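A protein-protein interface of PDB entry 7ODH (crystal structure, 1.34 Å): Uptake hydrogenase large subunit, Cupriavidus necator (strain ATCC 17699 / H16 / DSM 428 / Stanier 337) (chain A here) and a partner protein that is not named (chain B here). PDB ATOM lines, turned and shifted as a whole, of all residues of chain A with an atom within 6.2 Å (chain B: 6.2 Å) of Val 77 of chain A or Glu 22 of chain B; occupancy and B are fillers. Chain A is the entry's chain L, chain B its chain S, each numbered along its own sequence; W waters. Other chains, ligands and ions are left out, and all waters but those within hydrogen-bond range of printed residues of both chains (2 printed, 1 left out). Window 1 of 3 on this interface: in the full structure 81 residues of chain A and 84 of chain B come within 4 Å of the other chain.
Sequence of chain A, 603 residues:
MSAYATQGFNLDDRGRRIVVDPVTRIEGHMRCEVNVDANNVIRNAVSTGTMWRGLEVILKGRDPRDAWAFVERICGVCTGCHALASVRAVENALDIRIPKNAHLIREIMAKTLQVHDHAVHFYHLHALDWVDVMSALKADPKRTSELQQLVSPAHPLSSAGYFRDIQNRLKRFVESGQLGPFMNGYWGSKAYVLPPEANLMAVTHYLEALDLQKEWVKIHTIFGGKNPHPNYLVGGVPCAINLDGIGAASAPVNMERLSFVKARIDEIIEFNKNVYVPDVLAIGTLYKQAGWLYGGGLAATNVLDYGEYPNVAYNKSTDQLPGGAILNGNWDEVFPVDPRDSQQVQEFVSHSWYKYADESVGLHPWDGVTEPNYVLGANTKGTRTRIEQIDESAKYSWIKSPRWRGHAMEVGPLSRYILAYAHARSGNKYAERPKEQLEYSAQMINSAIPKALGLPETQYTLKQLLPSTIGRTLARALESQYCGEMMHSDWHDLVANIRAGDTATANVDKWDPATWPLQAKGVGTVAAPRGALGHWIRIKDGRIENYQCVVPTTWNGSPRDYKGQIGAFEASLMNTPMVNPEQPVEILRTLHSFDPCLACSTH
Among the printed residues, merely in contact across the chains: Glu 27 of chain A with Cys 17 of chain B (3.6 Å), Cys 75 of chain A with Cys 17 of chain B (3.7 Å), Gly 76 of chain A with CSO 19 of chain B (3.96 Å), Gly 76 of chain A with Glu 22 of chain B (3.6 Å), Val 77 of chain A with Cys 17 of chain B (3.9996 Å), Val 77 of chain A with Glu 22 of chain B (3.5 Å), His 116 of chain A with Glu 22 of chain B (3.6 Å), Pro 228 of chain A with CSO 19 of chain B (3.5 Å), Pro 228 of chain A with Glu 22 of chain B (3.6 Å) and Pro 228 of chain A with Ser 23 of chain B (3.8 Å).
Of the 17 printed residues of chain A, 9 touch a printed residue of chain B.
Of the 14 printed residues of chain B, 7 touch a printed residue of chain A.
Printed residues of chain B that touch a printed residue of chain A: Cys 17, Thr 18, CSO 19, Glu 22, Ser 23, Ile 25 and Arg 26.
Among the printed residues, 18 pairs touch across the chains.
Water W2 lies within hydrogen-bond range of the side-chain hydroxyl of Ser 23 of chain B (2.8 Å) and the backbone carbonyl oxygen of Asn 227 of chain A (2.8 Å).
Water W1 lies within hydrogen-bond range of the side-chain amide nitrogen (ND2) of Asn 227 of chain A (2.9 Å), a ring nitrogen (ND1) of His 116 of chain A (3.2 Å) and the guanidinium group (NH2) of Arg 26 of chain B (3.3 Å).
OE2 of Glu 27 of chain A lies within hydrogen-bond range of OG1 of Thr 18 of chain B (2.6 Å).
N of Gly 76 of chain A is in hydrogen-bond range of O of Cys 17 of chain B (2.8 Å).
NE2 of His 116 of chain A is in hydrogen-bond range of NH1 of Arg 26 of chain B (3.3 Å).
The side-chain amide nitrogen (NE2) of Gln 213 of chain A lies within hydrogen-bond range of the backbone carbonyl oxygen (O) of Ile 25 of chain B (2.8 Å).
The side-chain amide oxygen (OE1) of Gln 213 of chain A lies within hydrogen-bond range of the guanidinium group (NH1) of Arg 26 of chain B, at 3.0 Å.
OD1 of Asn 227 of chain A sits at hydrogen-bond distance from NH2 of Arg 26 of chain B, 2.8 Å away.
NE2 of His 229 of chain A lies close to SG of Cys 17 of chain B (3.3 Å).
A ring nitrogen (NE2) of His 229 of chain A sits close to OD of CSO 19 of chain B, at 3.4 Å.
Printed residues of chain B within 4 Å of Val 77 of chain A: Cys 17 and Glu 22.
Of chain A, only Gly 76, Val 77, His 116 and Pro 228 come within 4 Å of Glu 22 of chain B.
Printed residues of chain A within 4 Å of Arg 26 of chain B: His 116, Gln 213 and Asn 227.
Printed residues of chain A within 4 Å of Ile 25 of chain B: Gln 213.
Printed residues of chain A within 4 Å of Ser 23 of chain B: Pro 228.
Of the printed residues of chain A, CSO 19 of chain B touches Gly 76, Pro 228 and His 229.
Printed residues of chain A within 4 Å of Thr 18 of chain B: Glu 27.
The nearest printed residue of chain B that does not touch Val 77 of chain A is Thr 18 of chain B (4.05 Å).
The nearest printed residue of chain B that does not touch Glu 27 of chain A is Thr 47 of chain B (5.9 Å).
The side-chain carboxylate of Glu 27 of chain A sits close to the side-chain sulfur of Cys 597 of chain A (3.5 Å).
SG of Cys 75 of chain A lies close to N of Val 77 of chain A (3.4 Å).
OG1 of Thr 79 of chain A sits at hydrogen-bond distance from N of His 229 of chain A (2.7 Å).
A ring nitrogen (NE2) of His 116 of chain A lies within hydrogen-bond range of the side-chain amide oxygen (OE1) of Gln 213 of chain A (2.9 Å).
The side-chain carboxylate (OE1) of Glu 22 of chain B lies within salt-bridge range of the guanidinium group (NH1) of Arg 26 of chain B (2.8 Å).
OG of Ser 23 of chain B is in hydrogen-bond range of N of Ala 153 of chain B (3.3 Å).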
ATOM      1  N   GLU A  27     -10.761  -2.918 -26.063  1.00  0.00           N
ATOM      2  CA  GLU A  27     -11.932  -3.734 -26.431  1.00  0.00           C
ATOM      3  C   GLU A  27     -11.442  -4.861 -27.335  1.00  0.00           C
ATOM      4  O   GLU A  27     -10.677  -4.608 -28.284  1.00  0.00           O
ATOM      5  CB  GLU A  27     -13.018  -2.891 -27.087  1.00  0.00           C
ATOM      6  CG  GLU A  27     -14.316  -3.651 -27.286  1.00  0.00           C
ATOM      7  CD  GLU A  27     -14.254  -4.788 -28.291  1.00  0.00           C
ATOM      8  OE1 GLU A  27     -13.470  -4.672 -29.245  1.00  0.00           O
ATOM      9  OE2 GLU A  27     -15.000  -5.797 -28.118  1.00  0.00           O
ATOM     10  N   CYS A  75     -20.015  -3.375 -31.864  1.00  0.00           N
ATOM     11  CA  CYS A  75     -19.290  -2.869 -30.687  1.00  0.00           C
ATOM     12  C   CYS A  75     -20.214  -2.245 -29.648  1.00  0.00           C
ATOM     13  O   CYS A  75     -20.983  -1.339 -29.986  1.00  0.00           O
ATOM     14  CB  CYS A  75     -18.244  -1.857 -31.111  1.00  0.00           C
ATOM     15  SG  CYS A  75     -17.139  -1.463 -29.737  1.00  0.00           S
ATOM     16  N   GLY A  76     -20.038  -2.665 -28.399  1.00  0.00           N
ATOM     17  CA  GLY A  76     -20.793  -2.143 -27.253  1.00  0.00           C
ATOM     18  C   GLY A  76     -20.062  -1.032 -26.523  1.00  0.00           C
ATOM     19  O   GLY A  76     -20.644  -0.469 -25.590  1.00  0.00           O
ATOM     20  N   VAL A  77     -18.809  -0.769 -26.884  1.00  0.00           N
ATOM     21  CA  VAL A  77     -18.017   0.349 -26.313  1.00  0.00           C
ATOM     22  C   VAL A  77     -18.349   1.605 -27.119  1.00  0.00           C
ATOM     23  O   VAL A  77     -18.910   2.542 -26.539  1.00  0.00           O
ATOM     24  CB  VAL A  77     -16.516   0.030 -26.290  1.00  0.00           C
ATOM     25  CG1 VAL A  77     -15.724   1.201 -25.721  1.00  0.00           C
ATOM     26  CG2 VAL A  77     -16.248  -1.238 -25.497  1.00  0.00           C
ATOM     27  N   CYS A  78     -18.133   1.585 -28.435  1.00  0.00           N
ATOM     28  CA  CYS A  78     -18.564   2.700 -29.320  1.00  0.00           C
ATOM     29  C   CYS A  78     -20.044   2.491 -29.692  1.00  0.00           C
ATOM     30  O   CYS A  78     -20.424   2.502 -30.874  1.00  0.00           O
ATOM     31  CB  CYS A  78     -17.607   2.878 -30.496  1.00  0.00           C
ATOM     32  SG  CYS A  78     -17.414   1.429 -31.567  1.00  0.00           S
ATOM     33  N   THR A  79     -20.879   2.298 -28.681  1.00  0.00           N
ATOM     34  CA  THR A  79     -22.267   1.820 -28.870  1.00  0.00           C
ATOM     35  C   THR A  79     -23.109   2.906 -29.547  1.00  0.00           C
ATOM     36  O   THR A  79     -23.235   4.026 -29.011  1.00  0.00           O
ATOM     37  CB  THR A  79     -22.876   1.318 -27.559  1.00  0.00           C
ATOM     38  OG1 THR A  79     -24.189   0.858 -27.876  1.00  0.00           O
ATOM     39  CG2 THR A  79     -22.951   2.374 -26.480  1.00  0.00           C
ATOM     40  N   LEU A 113     -21.925   9.771 -26.668  1.00  0.00           N
ATOM     41  CA  LEU A 113     -21.011   8.618 -26.830  1.00  0.00           C
ATOM     42  C   LEU A 113     -19.563   9.112 -26.792  1.00  0.00           C
ATOM     43  O   LEU A 113     -18.739   8.487 -26.121  1.00  0.00           O
ATOM     44  CB  LEU A 113     -21.284   7.881 -28.136  1.00  0.00           C
ATOM     45  CG  LEU A 113     -20.314   6.728 -28.391  1.00  0.00           C
ATOM     46  CD1 LEU A 113     -20.457   5.659 -27.318  1.00  0.00           C
ATOM     47  CD2 LEU A 113     -20.496   6.138 -29.783  1.00  0.00           C
ATOM     48  N   HIS A 116     -18.570   9.835 -23.131  1.00  0.00           N
ATOM     49  CA  HIS A 116     -18.562   8.627 -22.283  1.00  0.00           C
ATOM     50  C   HIS A 116     -17.379   7.749 -22.681  1.00  0.00           C
ATOM     51  O   HIS A 116     -16.611   7.316 -21.817  1.00  0.00           O
ATOM     52  CB  HIS A 116     -19.880   7.879 -22.389  1.00  0.00           C
ATOM     53  CG  HIS A 116     -19.871   6.632 -21.588  1.00  0.00           C
ATOM     54  ND1 HIS A 116     -19.475   5.416 -22.110  1.00  0.00           N
ATOM     55  CD2 HIS A 116     -20.179   6.424 -20.292  1.00  0.00           C
ATOM     56  CE1 HIS A 116     -19.535   4.510 -21.152  1.00  0.00           C
ATOM     57  NE2 HIS A 116     -19.970   5.105 -20.026  1.00  0.00           N
ATOM     58  N   ASP A 117     -17.255   7.494 -23.969  1.00  0.00           N
ATOM     59  CA  ASP A 117     -16.211   6.600 -24.517  1.00  0.00           C
ATOM     60  C   ASP A 117     -14.829   7.193 -24.185  1.00  0.00           C
ATOM     61  O   ASP A 117     -13.972   6.474 -23.627  1.00  0.00           O
ATOM     62  CB  ASP A 117     -16.495   6.394 -26.000  1.00  0.00           C
ATOM     63  CG  ASP A 117     -15.869   5.159 -26.588  1.00  0.00           C
ATOM     64  OD1 ASP A 117     -14.849   4.716 -26.038  1.00  0.00           O
ATOM     65  OD2 ASP A 117     -16.395   4.678 -27.606  1.00  0.00           O
ATOM     66  N   VAL A 120     -14.109   7.243 -20.152  1.00  0.00           N
ATOM     67  CA  VAL A 120     -13.922   5.858 -19.643  1.00  0.00           C
ATOM     68  C   VAL A 120     -12.622   5.296 -20.224  1.00  0.00           C
ATOM     69  O   VAL A 120     -11.872   4.612 -19.498  1.00  0.00           O
ATOM     70  CB  VAL A 120     -15.126   4.958 -19.956  1.00  0.00           C
ATOM     71  CG1 VAL A 120     -14.814   3.493 -19.687  1.00  0.00           C
ATOM     72  CG2 VAL A 120     -16.350   5.400 -19.169  1.00  0.00           C
ATOM     73  N   GLN A 213     -19.804   7.932 -14.900  1.00  0.00           N
ATOM     74  CA  GLN A 213     -19.996   7.591 -16.334  1.00  0.00           C
ATOM     75  C   GLN A 213     -21.404   7.024 -16.555  1.00  0.00           C
ATOM     76  O   GLN A 213     -21.953   7.228 -17.642  1.00  0.00           O
ATOM     77  CB  GLN A 213     -18.903   6.665 -16.873  1.00  0.00           C
ATOM     78  CG  GLN A 213     -18.654   5.388 -16.081  1.00  0.00           C
ATOM     79  CD  GLN A 213     -19.712   4.317 -16.216  1.00  0.00           C
ATOM     80  OE1 GLN A 213     -20.251   4.055 -17.294  1.00  0.00           O
ATOM     81  NE2 GLN A 213     -19.974   3.633 -15.113  1.00  0.00           N
ATOM     82  N   ASN A 227     -28.853   1.965 -22.677  1.00  0.00           N
ATOM     83  CA  ASN A 227     -27.405   1.988 -22.955  1.00  0.00           C
ATOM     84  C   ASN A 227     -26.784   0.873 -22.134  1.00  0.00           C
ATOM     85  O   ASN A 227     -27.057   0.775 -20.943  1.00  0.00           O
ATOM     86  CB  ASN A 227     -26.794   3.350 -22.636  1.00  0.00           C
ATOM     87  CG  ASN A 227     -25.289   3.349 -22.778  1.00  0.00           C
ATOM     88  OD1 ASN A 227     -24.599   2.722 -21.974  1.00  0.00           O
ATOM     89  ND2 ASN A 227     -24.784   4.009 -23.811  1.00  0.00           N
ATOM     90  N   PRO A 228     -25.912   0.015 -22.703  1.00  0.00           N
ATOM     91  CA  PRO A 228     -25.534   0.038 -24.118  1.00  0.00           C
ATOM     92  C   PRO A 228     -26.636  -0.271 -25.138  1.00  0.00           C
ATOM     93  O   PRO A 228     -27.693  -0.783 -24.779  1.00  0.00           O
ATOM     94  CB  PRO A 228     -24.475  -1.072 -24.217  1.00  0.00           C
ATOM     95  CG  PRO A 228     -23.889  -1.142 -22.819  1.00  0.00           C
ATOM     96  CD  PRO A 228     -25.076  -0.899 -21.917  1.00  0.00           C
ATOM     97  N   HIS A 229     -26.324   0.041 -26.399  1.00  0.00           N
ATOM     98  CA  HIS A 229     -27.085  -0.322 -27.623  1.00  0.00           C
ATOM     99  C   HIS A 229     -28.448   0.371 -27.660  1.00  0.00           C
ATOM    100  O   HIS A 229     -29.501  -0.274 -27.753  1.00  0.00           O
ATOM    101  CB  HIS A 229     -27.179  -1.839 -27.756  1.00  0.00           C
ATOM    102  CG  HIS A 229     -25.887  -2.496 -28.085  1.00  0.00           C
ATOM    103  ND1 HIS A 229     -24.861  -1.840 -28.744  1.00  0.00           N
ATOM    104  CD2 HIS A 229     -25.468  -3.761 -27.878  1.00  0.00           C
ATOM    105  CE1 HIS A 229     -23.867  -2.678 -28.929  1.00  0.00           C
ATOM    106  NE2 HIS A 229     -24.219  -3.870 -28.434  1.00  0.00           N
ATOM    107  N   ARG A 530     -13.059   6.770 -32.214  1.00  0.00           N
ATOM    108  CA  ARG A 530     -11.679   6.339 -32.549  1.00  0.00           C
ATOM    109  C   ARG A 530     -11.254   6.808 -33.943  1.00  0.00           C
ATOM    110  O   ARG A 530     -10.107   6.544 -34.306  1.00  0.00           O
ATOM    111  CB  ARG A 530     -11.562   4.826 -32.403  1.00  0.00           C
ATOM    112  CG  ARG A 530     -11.619   4.380 -30.954  1.00  0.00           C
ATOM    113  CD  ARG A 530     -12.076   2.954 -30.783  1.00  0.00           C
ATOM    114  NE  ARG A 530     -12.243   2.700 -29.368  1.00  0.00           N
ATOM    115  CZ  ARG A 530     -13.298   3.056 -28.643  1.00  0.00           C
ATOM    116  NH1 ARG A 530     -13.277   2.857 -27.338  1.00  0.00           N
ATOM    117  NH2 ARG A 530     -14.371   3.575 -29.210  1.00  0.00           N
ATOM    118  N   ASP A 595      -6.737   3.984 -28.442  1.00  0.00           N
ATOM    119  CA  ASP A 595      -8.013   3.443 -27.934  1.00  0.00           C
ATOM    120  C   ASP A 595      -8.458   2.304 -28.853  1.00  0.00           C
ATOM    121  O   ASP A 595      -9.514   2.357 -29.488  1.00  0.00           O
ATOM    122  CB  ASP A 595      -8.987   4.610 -27.848  1.00  0.00           C
ATOM    123  CG  ASP A 595     -10.367   4.281 -27.363  1.00  0.00           C
ATOM    124  OD1 ASP A 595     -10.562   3.190 -26.763  1.00  0.00           O
ATOM    125  OD2 ASP A 595     -11.243   5.140 -27.596  1.00  0.00           O
ATOM    126  N   CYS A 597     -10.163  -0.656 -30.590  1.00  0.00           N
ATOM    127  CA  CYS A 597     -11.408  -1.434 -30.477  1.00  0.00           C
ATOM    128  C   CYS A 597     -11.360  -2.560 -31.498  1.00  0.00           C
ATOM    129  O   CYS A 597     -11.539  -2.313 -32.698  1.00  0.00           O
ATOM    130  CB  CYS A 597     -12.627  -0.565 -30.684  1.00  0.00           C
ATOM    131  SG  CYS A 597     -14.154  -1.443 -30.276  1.00  0.00           S
ATOM    132  N   CYS B  17     -18.988  -8.121 -28.399  1.00  0.00           N
ATOM    133  CA  CYS B  17     -18.940  -6.677 -28.691  1.00  0.00           C
ATOM    134  C   CYS B  17     -18.613  -5.896 -27.408  1.00  0.00           C
ATOM    135  O   CYS B  17     -18.388  -4.695 -27.521  1.00  0.00           O
ATOM    136  CB  CYS B  17     -20.249  -6.227 -29.341  1.00  0.00           C
ATOM    137  SG  CYS B  17     -21.515  -5.786 -28.133  1.00  0.00           S
ATOM    138  N   THR B  18     -18.579  -6.555 -26.240  1.00  0.00           N
ATOM    139  CA  THR B  18     -18.189  -5.980 -24.914  1.00  0.00           C
ATOM    140  C   THR B  18     -19.355  -5.168 -24.318  1.00  0.00           C
ATOM    141  O   THR B  18     -19.166  -4.462 -23.309  1.00  0.00           O
ATOM    142  CB  THR B  18     -16.865  -5.208 -25.019  1.00  0.00           C
ATOM    143  OG1 THR B  18     -15.942  -6.024 -25.741  1.00  0.00           O
ATOM    144  CG2 THR B  18     -16.258  -4.871 -23.675  1.00  0.00           C
ATOM    145  N   CSO B  19     -20.567  -5.318 -24.846  1.00  0.00           N
ATOM    146  CA  CSO B  19     -21.744  -4.605 -24.284  1.00  0.00           C
ATOM    147  CB  CSO B  19     -22.957  -4.731 -25.185  1.00  0.00           C
ATOM    148  SG  CSO B  19     -23.610  -6.414 -25.363  1.00  0.00           S
ATOM    149  C   CSO B  19     -22.043  -5.093 -22.863  1.00  0.00           C
ATOM    150  O   CSO B  19     -22.534  -4.294 -22.065  1.00  0.00           O
ATOM    151  OD  CSO B  19     -24.697  -6.636 -26.576  1.00  0.00           O
ATOM    152  N   CSO B  20     -21.765  -6.353 -22.542  1.00  0.00           N
ATOM    153  CA  CSO B  20     -22.107  -6.899 -21.207  1.00  0.00           C
ATOM    154  CB  CSO B  20     -22.071  -8.408 -21.207  1.00  0.00           C
ATOM    155  SG  CSO B  20     -23.153  -9.170 -22.461  1.00  0.00           S
ATOM    156  C   CSO B  20     -21.170  -6.274 -20.165  1.00  0.00           C
ATOM    157  O   CSO B  20     -21.654  -5.879 -19.088  1.00  0.00           O
ATOM    158  OD  CSO B  20     -22.205  -9.735 -23.686  1.00  0.00           O
ATOM    159  N   SER B  21     -19.872  -6.166 -20.461  1.00  0.00           N
ATOM    160  CA  SER B  21     -18.889  -5.480 -19.576  1.00  0.00           C
ATOM    161  C   SER B  21     -19.334  -4.034 -19.347  1.00  0.00           C
ATOM    162  O   SER B  21     -19.271  -3.538 -18.204  1.00  0.00           O
ATOM    163  CB  SER B  21     -17.494  -5.522 -20.151  1.00  0.00           C
ATOM    164  OG  SER B  21     -16.893  -6.791 -19.938  1.00  0.00           O
ATOM    165  N   GLU B  22     -19.756  -3.362 -20.411  1.00  0.00           N
ATOM    166  CA  GLU B  22     -20.225  -1.961 -20.309  1.00  0.00           C
ATOM    167  C   GLU B  22     -21.510  -1.910 -19.474  1.00  0.00           C
ATOM    168  O   GLU B  22     -21.613  -1.046 -18.599  1.00  0.00           O
ATOM    169  CB  GLU B  22     -20.423  -1.366 -21.698  1.00  0.00           C
ATOM    170  CG  GLU B  22     -19.130  -1.095 -22.412  1.00  0.00           C
ATOM    171  CD  GLU B  22     -18.394   0.159 -21.981  1.00  0.00           C
ATOM    172  OE1 GLU B  22     -18.931   0.943 -21.144  1.00  0.00           O
ATOM    173  OE2 GLU B  22     -17.303   0.389 -22.537  1.00  0.00           O
ATOM    174  N   SER B  23     -22.464  -2.799 -19.715  1.00  0.00           N
ATOM    175  CA  SER B  23     -23.726  -2.796 -18.941  1.00  0.00           C
ATOM    176  C   SER B  23     -23.406  -2.979 -17.451  1.00  0.00           C
ATOM    177  O   SER B  23     -23.962  -2.246 -16.605  1.00  0.00           O
ATOM    178  CB  SER B  23     -24.696  -3.818 -19.441  1.00  0.00           C
ATOM    179  OG  SER B  23     -25.962  -3.565 -18.871  1.00  0.00           O
ATOM    180  N   PHE B  24     -22.501  -3.900 -17.129  1.00  0.00           N
ATOM    181  CA  PHE B  24     -22.120  -4.198 -15.728  1.00  0.00           C
ATOM    182  C   PHE B  24     -21.771  -2.895 -14.994  1.00  0.00           C
ATOM    183  O   PHE B  24     -22.241  -2.685 -13.858  1.00  0.00           O
ATOM    184  CB  PHE B  24     -20.951  -5.180 -15.710  1.00  0.00           C
ATOM    185  CG  PHE B  24     -20.600  -5.703 -14.348  1.00  0.00           C
ATOM    186  CD1 PHE B  24     -21.352  -6.711 -13.774  1.00  0.00           C
ATOM    187  CD2 PHE B  24     -19.510  -5.208 -13.659  1.00  0.00           C
ATOM    188  CE1 PHE B  24     -21.026  -7.208 -12.527  1.00  0.00           C
ATOM    189  CE2 PHE B  24     -19.189  -5.701 -12.401  1.00  0.00           C
ATOM    190  CZ  PHE B  24     -19.950  -6.699 -11.840  1.00  0.00           C
ATOM    191  N   ILE B  25     -20.937  -2.043 -15.597  1.00  0.00           N
ATOM    192  CA  ILE B  25     -20.450  -0.814 -14.901  1.00  0.00           C
ATOM    193  C   ILE B  25     -21.530   0.277 -14.895  1.00  0.00           C
ATOM    194  O   ILE B  25     -21.307   1.298 -14.237  1.00  0.00           O
ATOM    195  CB  ILE B  25     -19.098  -0.307 -15.439  1.00  0.00           C
ATOM    196  CG1 ILE B  25     -19.162   0.204 -16.880  1.00  0.00           C
ATOM    197  CG2 ILE B  25     -18.040  -1.382 -15.270  1.00  0.00           C
ATOM    198  CD1 ILE B  25     -17.949   1.020 -17.277  1.00  0.00           C
ATOM    199  N   ARG B  26     -22.688   0.065 -15.521  1.00  0.00           N
ATOM    200  CA  ARG B  26     -23.823   1.019 -15.394  1.00  0.00           C
ATOM    201  C   ARG B  26     -24.622   0.757 -14.112  1.00  0.00           C
ATOM    202  O   ARG B  26     -25.528   1.541 -13.818  1.00  0.00           O
ATOM    203  CB  ARG B  26     -24.767   0.933 -16.589  1.00  0.00           C
ATOM    204  CG  ARG B  26     -24.087   1.174 -17.926  1.00  0.00           C
ATOM    205  CD  ARG B  26     -23.421   2.541 -18.109  1.00  0.00           C
ATOM    206  NE  ARG B  26     -23.112   2.588 -19.523  1.00  0.00           N
ATOM    207  CZ  ARG B  26     -21.973   2.178 -20.087  1.00  0.00           C
ATOM    208  NH1 ARG B  26     -20.882   1.970 -19.368  1.00  0.00           N
ATOM    209  NH2 ARG B  26     -21.919   2.072 -21.406  1.00  0.00           N
ATOM    210  N   SER B  27     -24.344  -0.319 -13.386  1.00  0.00           N
ATOM    211  CA  SER B  27     -25.167  -0.697 -12.215  1.00  0.00           C
ATOM    212  C   SER B  27     -25.154   0.436 -11.178  1.00  0.00           C
ATOM    213  O   SER B  27     -24.060   0.915 -10.826  1.00  0.00           O
ATOM    214  CB  SER B  27     -24.706  -1.982 -11.623  1.00  0.00           C
ATOM    215  OG  SER B  27     -25.601  -2.395 -10.610  1.00  0.00           O
ATOM    216  N   THR B  47     -10.703  -6.312 -20.177  1.00  0.00           N
ATOM    217  CA  THR B  47     -11.180  -4.912 -20.348  1.00  0.00           C
ATOM    218  C   THR B  47     -10.457  -3.972 -19.376  1.00  0.00           C
ATOM    219  O   THR B  47     -10.199  -2.821 -19.765  1.00  0.00           O
ATOM    220  CB  THR B  47     -12.702  -4.817 -20.160  1.00  0.00           C
ATOM    221  OG1 THR B  47     -13.310  -5.713 -21.090  1.00  0.00           O
ATOM    222  CG2 THR B  47     -13.250  -3.421 -20.373  1.00  0.00           C
ATOM    223  N   GLU B  76     -18.181 -13.708 -21.200  1.00  0.00           N
ATOM    224  CA  GLU B  76     -18.789 -12.772 -22.160  1.00  0.00           C
ATOM    225  C   GLU B  76     -18.360 -13.216 -23.550  1.00  0.00           C
ATOM    226  O   GLU B  76     -17.182 -13.527 -23.737  1.00  0.00           O
ATOM    227  CB  GLU B  76     -18.321 -11.360 -21.840  1.00  0.00           C
ATOM    228  CG  GLU B  76     -18.983 -10.278 -22.663  1.00  0.00           C
ATOM    229  CD  GLU B  76     -18.644  -8.889 -22.146  1.00  0.00           C
ATOM    230  OE1 GLU B  76     -17.953  -8.806 -21.112  1.00  0.00           O
ATOM    231  OE2 GLU B  76     -19.094  -7.908 -22.749  1.00  0.00           O
ATOM    232  N   ALA B 153     -28.180  -3.787 -16.398  1.00  0.00           N
ATOM    233  CA  ALA B 153     -27.034  -3.679 -15.469  1.00  0.00           C
ATOM    234  C   ALA B 153     -27.391  -4.329 -14.128  1.00  0.00           C
ATOM    235  O   ALA B 153     -26.598  -5.142 -13.623  1.00  0.00           O
ATOM    236  CB  ALA B 153     -26.646  -2.238 -15.286  1.00  0.00           C
HETATM  237  O   HOH W   1     -21.855   4.219 -23.921  1.00  0.00           O
HETATM  238  O   HOH W   2     -26.878  -0.892 -18.656  1.00  0.00           O
